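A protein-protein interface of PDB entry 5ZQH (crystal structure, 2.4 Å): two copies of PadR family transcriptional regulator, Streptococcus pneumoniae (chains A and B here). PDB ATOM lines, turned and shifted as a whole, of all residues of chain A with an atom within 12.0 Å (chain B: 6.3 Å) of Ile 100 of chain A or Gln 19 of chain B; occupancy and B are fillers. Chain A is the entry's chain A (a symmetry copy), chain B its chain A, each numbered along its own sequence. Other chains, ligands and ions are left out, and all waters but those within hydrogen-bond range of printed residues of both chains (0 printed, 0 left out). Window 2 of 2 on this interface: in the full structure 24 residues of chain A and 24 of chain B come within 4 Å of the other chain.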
ATOM      1  N   GLN A  89       6.094 -21.774   3.596  1.00  0.00           N
ATOM      2  CA  GLN A  89       4.909 -20.960   3.876  1.00  0.00           C
ATOM      3  C   GLN A  89       4.212 -21.375   5.172  1.00  0.00           C
ATOM      4  O   GLN A  89       3.710 -20.521   5.894  1.00  0.00           O
ATOM      5  CB  GLN A  89       3.928 -20.987   2.706  1.00  0.00           C
ATOM      6  CG  GLN A  89       3.021 -19.769   2.652  1.00  0.00           C
ATOM      7  CD  GLN A  89       2.255 -19.642   1.350  1.00  0.00           C
ATOM      8  OE1 GLN A  89       2.234 -18.573   0.742  1.00  0.00           O
ATOM      9  NE2 GLN A  89       1.614 -20.726   0.920  1.00  0.00           N
ATOM     10  N   TRP A  90       4.195 -22.675   5.467  1.00  0.00           N
ATOM     11  CA  TRP A  90       3.611 -23.165   6.714  1.00  0.00           C
ATOM     12  C   TRP A  90       4.427 -22.726   7.937  1.00  0.00           C
ATOM     13  O   TRP A  90       3.845 -22.251   8.918  1.00  0.00           O
ATOM     14  CB  TRP A  90       3.395 -24.687   6.711  1.00  0.00           C
ATOM     15  CG  TRP A  90       2.790 -25.147   7.995  1.00  0.00           C
ATOM     16  CD1 TRP A  90       3.439 -25.750   9.044  1.00  0.00           C
ATOM     17  CD2 TRP A  90       1.426 -24.991   8.403  1.00  0.00           C
ATOM     18  NE1 TRP A  90       2.555 -26.000  10.070  1.00  0.00           N
ATOM     19  CE2 TRP A  90       1.313 -25.545   9.706  1.00  0.00           C
ATOM     20  CE3 TRP A  90       0.284 -24.449   7.792  1.00  0.00           C
ATOM     21  CZ2 TRP A  90       0.101 -25.572  10.409  1.00  0.00           C
ATOM     22  CZ3 TRP A  90      -0.925 -24.479   8.489  1.00  0.00           C
ATOM     23  CH2 TRP A  90      -1.003 -25.037   9.790  1.00  0.00           C
ATOM     24  N   ASP A  91       5.753 -22.888   7.866  1.00  0.00           N
ATOM     25  CA  ASP A  91       6.680 -22.430   8.908  1.00  0.00           C
ATOM     26  C   ASP A  91       6.597 -20.917   9.145  1.00  0.00           C
ATOM     27  O   ASP A  91       6.634 -20.467  10.296  1.00  0.00           O
ATOM     28  CB  ASP A  91       8.124 -22.824   8.564  1.00  0.00           C
ATOM     29  CG  ASP A  91       8.419 -24.304   8.812  1.00  0.00           C
ATOM     30  OD1 ASP A  91       7.506 -25.155   8.684  1.00  0.00           O
ATOM     31  OD2 ASP A  91       9.590 -24.623   9.125  1.00  0.00           O
ATOM     32  N   ASP A  92       6.480 -20.152   8.053  1.00  0.00           N
ATOM     33  CA  ASP A  92       6.393 -18.690   8.099  1.00  0.00           C
ATOM     34  C   ASP A  92       5.090 -18.229   8.758  1.00  0.00           C
ATOM     35  O   ASP A  92       5.123 -17.442   9.704  1.00  0.00           O
ATOM     36  CB  ASP A  92       6.568 -18.085   6.692  1.00  0.00           C
ATOM     37  CG  ASP A  92       6.370 -16.564   6.658  1.00  0.00           C
ATOM     38  OD1 ASP A  92       7.126 -15.823   7.331  1.00  0.00           O
ATOM     39  OD2 ASP A  92       5.461 -16.107   5.934  1.00  0.00           O
ATOM     40  N   LEU A  93       3.962 -18.746   8.272  1.00  0.00           N
ATOM     41  CA  LEU A  93       2.644 -18.341   8.762  1.00  0.00           C
ATOM     42  C   LEU A  93       2.358 -18.803  10.195  1.00  0.00           C
ATOM     43  O   LEU A  93       1.664 -18.102  10.933  1.00  0.00           O
ATOM     44  CB  LEU A  93       1.527 -18.761   7.790  1.00  0.00           C
ATOM     45  CG  LEU A  93       1.523 -18.118   6.389  1.00  0.00           C
ATOM     46  CD1 LEU A  93       0.568 -18.852   5.456  1.00  0.00           C
ATOM     47  CD2 LEU A  93       1.196 -16.630   6.430  1.00  0.00           C
ATOM     48  N   SER A  94       2.918 -19.952  10.588  1.00  0.00           N
ATOM     49  CA  SER A  94       2.797 -20.467  11.961  1.00  0.00           C
ATOM     50  C   SER A  94       3.357 -19.498  13.004  1.00  0.00           C
ATOM     51  O   SER A  94       2.676 -19.212  13.991  1.00  0.00           O
ATOM     52  CB  SER A  94       3.450 -21.848  12.106  1.00  0.00           C
ATOM     53  OG  SER A  94       2.834 -22.798  11.251  1.00  0.00           O
ATOM     54  N   GLN A  95       4.574 -18.992  12.774  1.00  0.00           N
ATOM     55  CA  GLN A  95       5.208 -18.039  13.698  1.00  0.00           C
ATOM     56  C   GLN A  95       4.573 -16.641  13.692  1.00  0.00           C
ATOM     57  O   GLN A  95       4.574 -15.954  14.716  1.00  0.00           O
ATOM     58  CB  GLN A  95       6.743 -17.995  13.541  1.00  0.00           C
ATOM     59  CG  GLN A  95       7.291 -17.209  12.353  1.00  0.00           C
ATOM     60  CD  GLN A  95       8.730 -16.748  12.562  1.00  0.00           C
ATOM     61  OE1 GLN A  95       9.612 -17.542  12.894  1.00  0.00           O
ATOM     62  NE2 GLN A  95       8.974 -15.459  12.361  1.00  0.00           N
ATOM     63  N   LYS A  96       4.017 -16.246  12.544  1.00  0.00           N
ATOM     64  CA  LYS A  96       3.221 -15.016  12.424  1.00  0.00           C
ATOM     65  C   LYS A  96       1.923 -15.094  13.239  1.00  0.00           C
ATOM     66  O   LYS A  96       1.586 -14.154  13.967  1.00  0.00           O
ATOM     67  CB  LYS A  96       2.876 -14.727  10.956  1.00  0.00           C
ATOM     68  CG  LYS A  96       4.033 -14.253  10.095  1.00  0.00           C
ATOM     69  CD  LYS A  96       3.570 -14.079   8.660  1.00  0.00           C
ATOM     70  CE  LYS A  96       4.645 -13.446   7.801  1.00  0.00           C
ATOM     71  NZ  LYS A  96       4.099 -13.046   6.475  1.00  0.00           N
ATOM     72  N   VAL A  97       1.208 -16.217  13.089  1.00  0.00           N
ATOM     73  CA  VAL A  97      -0.075 -16.471  13.752  1.00  0.00           C
ATOM     74  C   VAL A  97       0.101 -16.554  15.272  1.00  0.00           C
ATOM     75  O   VAL A  97      -0.697 -15.969  16.017  1.00  0.00           O
ATOM     76  CB  VAL A  97      -0.795 -17.719  13.154  1.00  0.00           C
ATOM     77  CG1 VAL A  97      -1.920 -18.225  14.045  1.00  0.00           C
ATOM     78  CG2 VAL A  97      -1.360 -17.397  11.781  1.00  0.00           C
ATOM     79  N   GLU A  98       1.148 -17.264  15.708  1.00  0.00           N
ATOM     80  CA  GLU A  98       1.576 -17.320  17.117  1.00  0.00           C
ATOM     81  C   GLU A  98       1.726 -15.915  17.720  1.00  0.00           C
ATOM     82  O   GLU A  98       1.159 -15.632  18.783  1.00  0.00           O
ATOM     83  CB  GLU A  98       2.878 -18.134  17.246  1.00  0.00           C
ATOM     84  CG  GLU A  98       3.655 -17.965  18.547  1.00  0.00           C
ATOM     85  CD  GLU A  98       3.259 -18.972  19.610  1.00  0.00           C
ATOM     86  OE1 GLU A  98       3.809 -20.099  19.588  1.00  0.00           O
ATOM     87  OE2 GLU A  98       2.406 -18.636  20.470  1.00  0.00           O
ATOM     88  N   GLY A  99       2.468 -15.053  17.020  1.00  0.00           N
ATOM     89  CA  GLY A  99       2.694 -13.661  17.420  1.00  0.00           C
ATOM     90  C   GLY A  99       1.437 -12.823  17.575  1.00  0.00           C
ATOM     91  O   GLY A  99       1.344 -12.011  18.493  1.00  0.00           O
ATOM     92  N   ILE A 100       0.474 -13.029  16.678  1.00  0.00           N
ATOM     93  CA  ILE A 100      -0.812 -12.309  16.691  1.00  0.00           C
ATOM     94  C   ILE A 100      -1.717 -12.808  17.829  1.00  0.00           C
ATOM     95  O   ILE A 100      -2.315 -12.002  18.556  1.00  0.00           O
ATOM     96  CB  ILE A 100      -1.517 -12.401  15.309  1.00  0.00           C
ATOM     97  CG1 ILE A 100      -0.697 -11.641  14.258  1.00  0.00           C
ATOM     98  CG2 ILE A 100      -2.943 -11.855  15.363  1.00  0.00           C
ATOM     99  CD1 ILE A 100      -0.886 -12.101  12.827  1.00  0.00           C
ATOM    100  N   LYS A 101      -1.791 -14.134  17.967  1.00  0.00           N
ATOM    101  CA  LYS A 101      -2.581 -14.823  18.993  1.00  0.00           C
ATOM    102  C   LYS A 101      -2.302 -14.299  20.403  1.00  0.00           C
ATOM    103  O   LYS A 101      -3.242 -14.060  21.165  1.00  0.00           O
ATOM    104  CB  LYS A 101      -2.324 -16.336  18.911  1.00  0.00           C
ATOM    105  CG  LYS A 101      -3.149 -17.212  19.843  1.00  0.00           C
ATOM    106  CD  LYS A 101      -2.923 -18.676  19.501  1.00  0.00           C
ATOM    107  CE  LYS A 101      -2.878 -19.548  20.746  1.00  0.00           C
ATOM    108  NZ  LYS A 101      -2.248 -20.867  20.461  1.00  0.00           N
ATOM    109  N   ASN A 102      -1.020 -14.109  20.723  1.00  0.00           N
ATOM    110  CA  ASN A 102      -0.579 -13.631  22.039  1.00  0.00           C
ATOM    111  C   ASN A 102      -0.385 -12.115  22.060  1.00  0.00           C
ATOM    112  O   ASN A 102      -1.161 -11.363  21.462  1.00  0.00           O
ATOM    113  CB  ASN A 102       0.724 -14.325  22.469  1.00  0.00           C
ATOM    114  CG  ASN A 102       0.801 -15.788  22.040  1.00  0.00           C
ATOM    115  OD1 ASN A 102      -0.216 -16.459  21.856  1.00  0.00           O
ATOM    116  ND2 ASN A 102       2.018 -16.287  21.881  1.00  0.00           N
ATOM    117  N   CYS B  12      -6.380 -13.726  10.590  1.00  0.00           N
ATOM    118  CA  CYS B  12      -5.557 -12.706  11.273  1.00  0.00           C
ATOM    119  C   CYS B  12      -6.186 -11.308  11.271  1.00  0.00           C
ATOM    120  O   CYS B  12      -6.230 -10.663  12.318  1.00  0.00           O
ATOM    121  CB  CYS B  12      -4.121 -12.674  10.722  1.00  0.00           C
ATOM    122  SG  CYS B  12      -3.146 -14.148  11.122  1.00  0.00           S
ATOM    123  N   LEU B  14      -9.445 -10.622  10.823  1.00  0.00           N
ATOM    124  CA  LEU B  14     -10.618 -10.826  11.676  1.00  0.00           C
ATOM    125  C   LEU B  14     -10.295 -10.774  13.178  1.00  0.00           C
ATOM    126  O   LEU B  14     -11.009 -10.110  13.940  1.00  0.00           O
ATOM    127  CB  LEU B  14     -11.305 -12.149  11.307  1.00  0.00           C
ATOM    128  CG  LEU B  14     -12.722 -12.247  10.712  1.00  0.00           C
ATOM    129  CD1 LEU B  14     -13.269 -10.968  10.087  1.00  0.00           C
ATOM    130  CD2 LEU B  14     -12.799 -13.417   9.735  1.00  0.00           C
ATOM    131  N   ASP B  15      -9.216 -11.453  13.582  1.00  0.00           N
ATOM    132  CA  ASP B  15      -8.750 -11.461  14.978  1.00  0.00           C
ATOM    133  C   ASP B  15      -8.321 -10.075  15.462  1.00  0.00           C
ATOM    134  O   ASP B  15      -8.707  -9.660  16.557  1.00  0.00           O
ATOM    135  CB  ASP B  15      -7.620 -12.481  15.173  1.00  0.00           C
ATOM    136  CG  ASP B  15      -7.311 -12.756  16.645  1.00  0.00           C
ATOM    137  OD1 ASP B  15      -8.195 -13.272  17.366  1.00  0.00           O
ATOM    138  OD2 ASP B  15      -6.173 -12.469  17.072  1.00  0.00           O
ATOM    139  N   MET B  16      -7.542  -9.371  14.636  1.00  0.00           N
ATOM    140  CA  MET B  16      -7.072  -8.011  14.928  1.00  0.00           C
ATOM    141  C   MET B  16      -8.209  -7.013  15.145  1.00  0.00           C
ATOM    142  O   MET B  16      -8.136  -6.186  16.055  1.00  0.00           O
ATOM    143  CB  MET B  16      -6.131  -7.510  13.832  1.00  0.00           C
ATOM    144  CG  MET B  16      -4.742  -8.111  13.894  1.00  0.00           C
ATOM    145  SD  MET B  16      -3.752  -7.624  12.473  1.00  0.00           S
ATOM    146  CE  MET B  16      -2.219  -8.478  12.844  1.00  0.00           C
ATOM    147  N   ILE B  17      -9.246  -7.114  14.310  1.00  0.00           N
ATOM    148  CA  ILE B  17     -10.477  -6.316  14.409  1.00  0.00           C
ATOM    149  C   ILE B  17     -11.258  -6.651  15.694  1.00  0.00           C
ATOM    150  O   ILE B  17     -11.877  -5.768  16.299  1.00  0.00           O
ATOM    151  CB  ILE B  17     -11.338  -6.477  13.127  1.00  0.00           C
ATOM    152  CG1 ILE B  17     -10.714  -5.695  11.968  1.00  0.00           C
ATOM    153  CG2 ILE B  17     -12.776  -6.017  13.325  1.00  0.00           C
ATOM    154  CD1 ILE B  17     -11.091  -6.209  10.590  1.00  0.00           C
ATOM    155  N   GLY B  18     -11.203  -7.918  16.104  1.00  0.00           N
ATOM    156  CA  GLY B  18     -11.768  -8.377  17.380  1.00  0.00           C
ATOM    157  C   GLY B  18     -11.094  -7.830  18.628  1.00  0.00           C
ATOM    158  O   GLY B  18     -11.782  -7.434  19.576  1.00  0.00           O
ATOM    159  N   GLN B  19      -9.755  -7.815  18.626  1.00  0.00           N
ATOM    160  CA  GLN B  19      -8.949  -7.292  19.742  1.00  0.00           C
ATOM    161  C   GLN B  19      -9.199  -5.802  19.953  1.00  0.00           C
ATOM    162  O   GLN B  19      -9.475  -5.358  21.070  1.00  0.00           O
ATOM    163  CB  GLN B  19      -7.452  -7.488  19.482  1.00  0.00           C
ATOM    164  CG  GLN B  19      -6.963  -8.920  19.310  1.00  0.00           C
ATOM    165  CD  GLN B  19      -5.515  -8.984  18.827  1.00  0.00           C
ATOM    166  OE1 GLN B  19      -4.782  -7.981  18.872  1.00  0.00           O
ATOM    167  NE2 GLN B  19      -5.094 -10.162  18.362  1.00  0.00           N
ATOM    168  N   LYS B  20      -9.086  -5.045  18.861  1.00  0.00           N
ATOM    169  CA  LYS B  20      -9.278  -3.601  18.861  1.00  0.00           C
ATOM    170  C   LYS B  20      -9.872  -3.145  17.529  1.00  0.00           C
ATOM    171  O   LYS B  20      -9.384  -3.502  16.452  1.00  0.00           O
ATOM    172  CB  LYS B  20      -7.955  -2.876  19.134  1.00  0.00           C
ATOM    173  CG  LYS B  20      -8.108  -1.403  19.472  1.00  0.00           C
ATOM    174  CD  LYS B  20      -6.860  -0.626  19.088  1.00  0.00           C
ATOM    175  CE  LYS B  20      -7.123   0.876  19.035  1.00  0.00           C
ATOM    176  NZ  LYS B  20      -7.905   1.316  17.835  1.00  0.00           N
ATOM    177  N   GLU B  21     -10.942  -2.362  17.638  1.00  0.00           N
ATOM    178  CA  GLU B  21     -11.582  -1.655  16.535  1.00  0.00           C
ATOM    179  C   GLU B  21     -10.533  -0.831  15.767  1.00  0.00           C
ATOM    180  O   GLU B  21      -9.915   0.078  16.337  1.00  0.00           O
ATOM    181  CB  GLU B  21     -12.652  -0.745  17.138  1.00  0.00           C
ATOM    182  CG  GLU B  21     -13.764  -0.315  16.206  1.00  0.00           C
ATOM    183  CD  GLU B  21     -14.878   0.411  16.936  1.00  0.00           C
ATOM    184  OE1 GLU B  21     -15.245  -0.023  18.058  1.00  0.00           O
ATOM    185  OE2 GLU B  21     -15.387   1.421  16.385  1.00  0.00           O
ATOM    186  N   ARG B  22     -10.322  -1.169  14.492  1.00  0.00           N
ATOM    187  CA  ARG B  22      -9.252  -0.564  13.679  1.00  0.00           C
ATOM    188  C   ARG B  22      -9.715  -0.060  12.314  1.00  0.00           C
ATOM    189  O   ARG B  22     -10.601  -0.662  11.699  1.00  0.00           O
ATOM    190  CB  ARG B  22      -8.116  -1.570  13.470  1.00  0.00           C
ATOM    191  CG  ARG B  22      -7.120  -1.648  14.615  1.00  0.00           C
ATOM    192  CD  ARG B  22      -5.879  -2.427  14.207  1.00  0.00           C
ATOM    193  NE  ARG B  22      -4.961  -2.618  15.328  1.00  0.00           N
ATOM    194  CZ  ARG B  22      -4.933  -3.685  16.127  1.00  0.00           C
ATOM    195  NH1 ARG B  22      -5.777  -4.701  15.957  1.00  0.00           N
ATOM    196  NH2 ARG B  22      -4.046  -3.731  17.112  1.00  0.00           N
ATOM    197  N   THR B  30      -0.377  -2.844  11.525  1.00  0.00           N
ATOM    198  CA  THR B  30      -0.423  -3.923  12.523  1.00  0.00           C
ATOM    199  C   THR B  30      -0.037  -5.265  11.892  1.00  0.00           C
ATOM    200  O   THR B  30       0.619  -6.086  12.528  1.00  0.00           O
ATOM    201  CB  THR B  30      -1.816  -3.999  13.193  1.00  0.00           C
ATOM    202  OG1 THR B  30      -2.186  -2.694  13.655  1.00  0.00           O
ATOM    203  CG2 THR B  30      -1.827  -4.950  14.388  1.00  0.00           C
ATOM    204  N   LEU B  31      -0.427  -5.450  10.631  1.00  0.00           N
ATOM    205  CA  LEU B  31      -0.143  -6.654   9.850  1.00  0.00           C
ATOM    206  C   LEU B  31       1.356  -6.739   9.513  1.00  0.00           C
ATOM    207  O   LEU B  31       1.972  -7.798   9.682  1.00  0.00           O
ATOM    208  CB  LEU B  31      -1.008  -6.651   8.581  1.00  0.00           C
ATOM    209  CG  LEU B  31      -1.902  -7.787   8.062  1.00  0.00           C
ATOM    210  CD1 LEU B  31      -2.501  -8.712   9.113  1.00  0.00           C
ATOM    211  CD2 LEU B  31      -3.017  -7.165   7.243  1.00  0.00           C
ATOM    212  N   ALA B  34       3.399  -7.634  12.535  1.00  0.00           N
ATOM    213  CA  ALA B  34       3.207  -9.039  12.902  1.00  0.00           C
ATOM    214  C   ALA B  34       4.075  -9.976  12.055  1.00  0.00           C
ATOM    215  O   ALA B  34       4.254 -11.151  12.404  1.00  0.00           O
ATOM    216  CB  ALA B  34       1.739  -9.420  12.791  1.00  0.00           C
ATOM    217  N   PHE B  36       4.019  -9.581   8.243  1.00  0.00           N
ATOM    218  CA  PHE B  36       3.597  -9.407   6.858  1.00  0.00           C
ATOM    219  C   PHE B  36       4.300  -8.190   6.223  1.00  0.00           C
ATOM    220  O   PHE B  36       3.671  -7.191   5.858  1.00  0.00           O
ATOM    221  CB  PHE B  36       2.060  -9.324   6.771  1.00  0.00           C
ATOM    222  CG  PHE B  36       1.347 -10.552   7.292  1.00  0.00           C
ATOM    223  CD1 PHE B  36       1.098 -11.643   6.453  1.00  0.00           C
ATOM    224  CD2 PHE B  36       0.920 -10.626   8.624  1.00  0.00           C
ATOM    225  CE1 PHE B  36       0.443 -12.777   6.931  1.00  0.00           C
ATOM    226  CE2 PHE B  36       0.269 -11.755   9.106  1.00  0.00           C
ATOM    227  CZ  PHE B  36       0.027 -12.830   8.258  1.00  0.00           C
ATOM    228  N   LEU B  75     -16.105  -6.111  14.624  1.00  0.00           N
ATOM    229  CA  LEU B  75     -16.765  -7.384  14.318  1.00  0.00           C
ATOM    230  C   LEU B  75     -18.286  -7.366  14.498  1.00  0.00           C
ATOM    231  O   LEU B  75     -18.807  -6.809  15.464  1.00  0.00           O
ATOM    232  CB  LEU B  75     -16.159  -8.529  15.141  1.00  0.00           C
ATOM    233  CG  LEU B  75     -14.747  -9.057  14.860  1.00  0.00           C
ATOM    234  CD1 LEU B  75     -14.445 -10.171  15.843  1.00  0.00           C
ATOM    235  CD2 LEU B  75     -14.569  -9.564  13.435  1.00  0.00           C
ATOM    236  N   TRP B  87      -9.637 -19.993  14.932  1.00  0.00           N
ATOM    237  CA  TRP B  87      -8.710 -20.465  15.966  1.00  0.00           C
ATOM    238  C   TRP B  87      -8.831 -21.949  16.276  1.00  0.00           C
ATOM    239  O   TRP B  87      -7.827 -22.600  16.567  1.00  0.00           O
ATOM    240  CB  TRP B  87      -8.797 -19.630  17.247  1.00  0.00           C
ATOM    241  CG  TRP B  87      -8.192 -18.258  17.102  1.00  0.00           C
ATOM    242  CD1 TRP B  87      -8.810 -17.063  17.336  1.00  0.00           C
ATOM    243  CD2 TRP B  87      -6.856 -17.940  16.674  1.00  0.00           C
ATOM    244  NE1 TRP B  87      -7.946 -16.022  17.095  1.00  0.00           N
ATOM    245  CE2 TRP B  87      -6.741 -16.528  16.686  1.00  0.00           C
ATOM    246  CE3 TRP B  87      -5.744 -18.710  16.292  1.00  0.00           C
ATOM    247  CZ2 TRP B  87      -5.558 -15.864  16.324  1.00  0.00           C
ATOM    248  CZ3 TRP B  87      -4.565 -18.050  15.935  1.00  0.00           C
ATOM    249  CH2 TRP B  87      -4.483 -16.639  15.956  1.00  0.00           C
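The side-chain amide nitrogen of Gln 19 of chain B sits at hydrogen-bond distance from the backbone carbonyl oxygen of Ile 100 of chain A, at 3.3 Å.
OD2 of Asp 15 of chain B lies within hydrogen-bond range of NE2 of Gln 19 of chain B, 2.9 Å away.
OD1 of Asp 15 of chain B lies within hydrogen-bond range of NE1 of Trp 87 of chain B.
O of Met 16 of chain B lies within hydrogen-bond range of NH1 of Arg 22 of chain B (2.8 Å).
N of Phe 36 of chain B sits at hydrogen-bond distance from O of Leu 31 of chain B (3.1 Å).
OD2 of Asp 92 of chain A is in salt-bridge range of NZ of Lys 96 of chain A (3.4 Å).
Leu 93 of chain A touches Phe 36 of chain B (CD2 to CE1, 3.96 Å).
Lys 96 of chain A touches Ala 34 of chain B (CG to O, 3.9 Å).
Phe 36 of chain B touches Lys 96 of chain A.
Val 97 of chain A touches Cys 12 of chain B (CG2 to SG, 3.8 Å).
Trp 87 of chain B touches Val 97 of chain A (CZ3 to CG1, 3.3 Å).
Cys 12 of chain B touches Ile 100 of chain A (SG to CD1, 3.5 Å).
Ile 100 of chain A touches Met 16 of chain B (CG1 to CE, 3.8 Å).
Ala 34 of chain B touches Ile 100 of chain A (CB to CG1, 3.6 Å).
Ile 100 of chain A touches Phe 36 of chain B (CD1 to CE2, 3.9 Å).
Trp 87 of chain B touches Lys 101 of chain A (CH2 to CB, 3.7 Å).
Of the printed residues of chain B, Ile 100 of chain A touches Cys 12, Asp 15, Met 16, Gln 19, Ala 34 and Phe 36.
Of the printed residues of chain A, Gln 19 of chain B touches Ile 100.
Of the printed residues of chain A, Asp 15 of chain B touches Ile 100.
Met 16 of chain B touches one residue of chain A.
No residue of chain A comes within 4 Å of Lys 20 of chain B.
No residue of chain A comes within 4 Å of Leu 31 of chain B.
Of the printed residues of chain B, Lys 96 of chain A touches Ala 34 (3.9 Å) and Phe 36 (3.3 Å).
Of the printed residues of chain A, Trp 87 of chain B touches Val 97 (3.3 Å) and Lys 101 (3.7 Å).
The nearest printed residue of chain A that does not touch Gln 19 of chain B is Lys 101 of chain A (5.1 Å).
The nearest printed residue of chain B that does not touch Lys 101 of chain A is Asp 15 of chain B (4.7 Å).
Of the 16 printed residues of chain B, 7 touch a printed residue of chain A.
No position is printed for both chains.
Of the 12 pairs that touch across the chains among the printed residues, none has its exchanged pair printed and touching as well.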
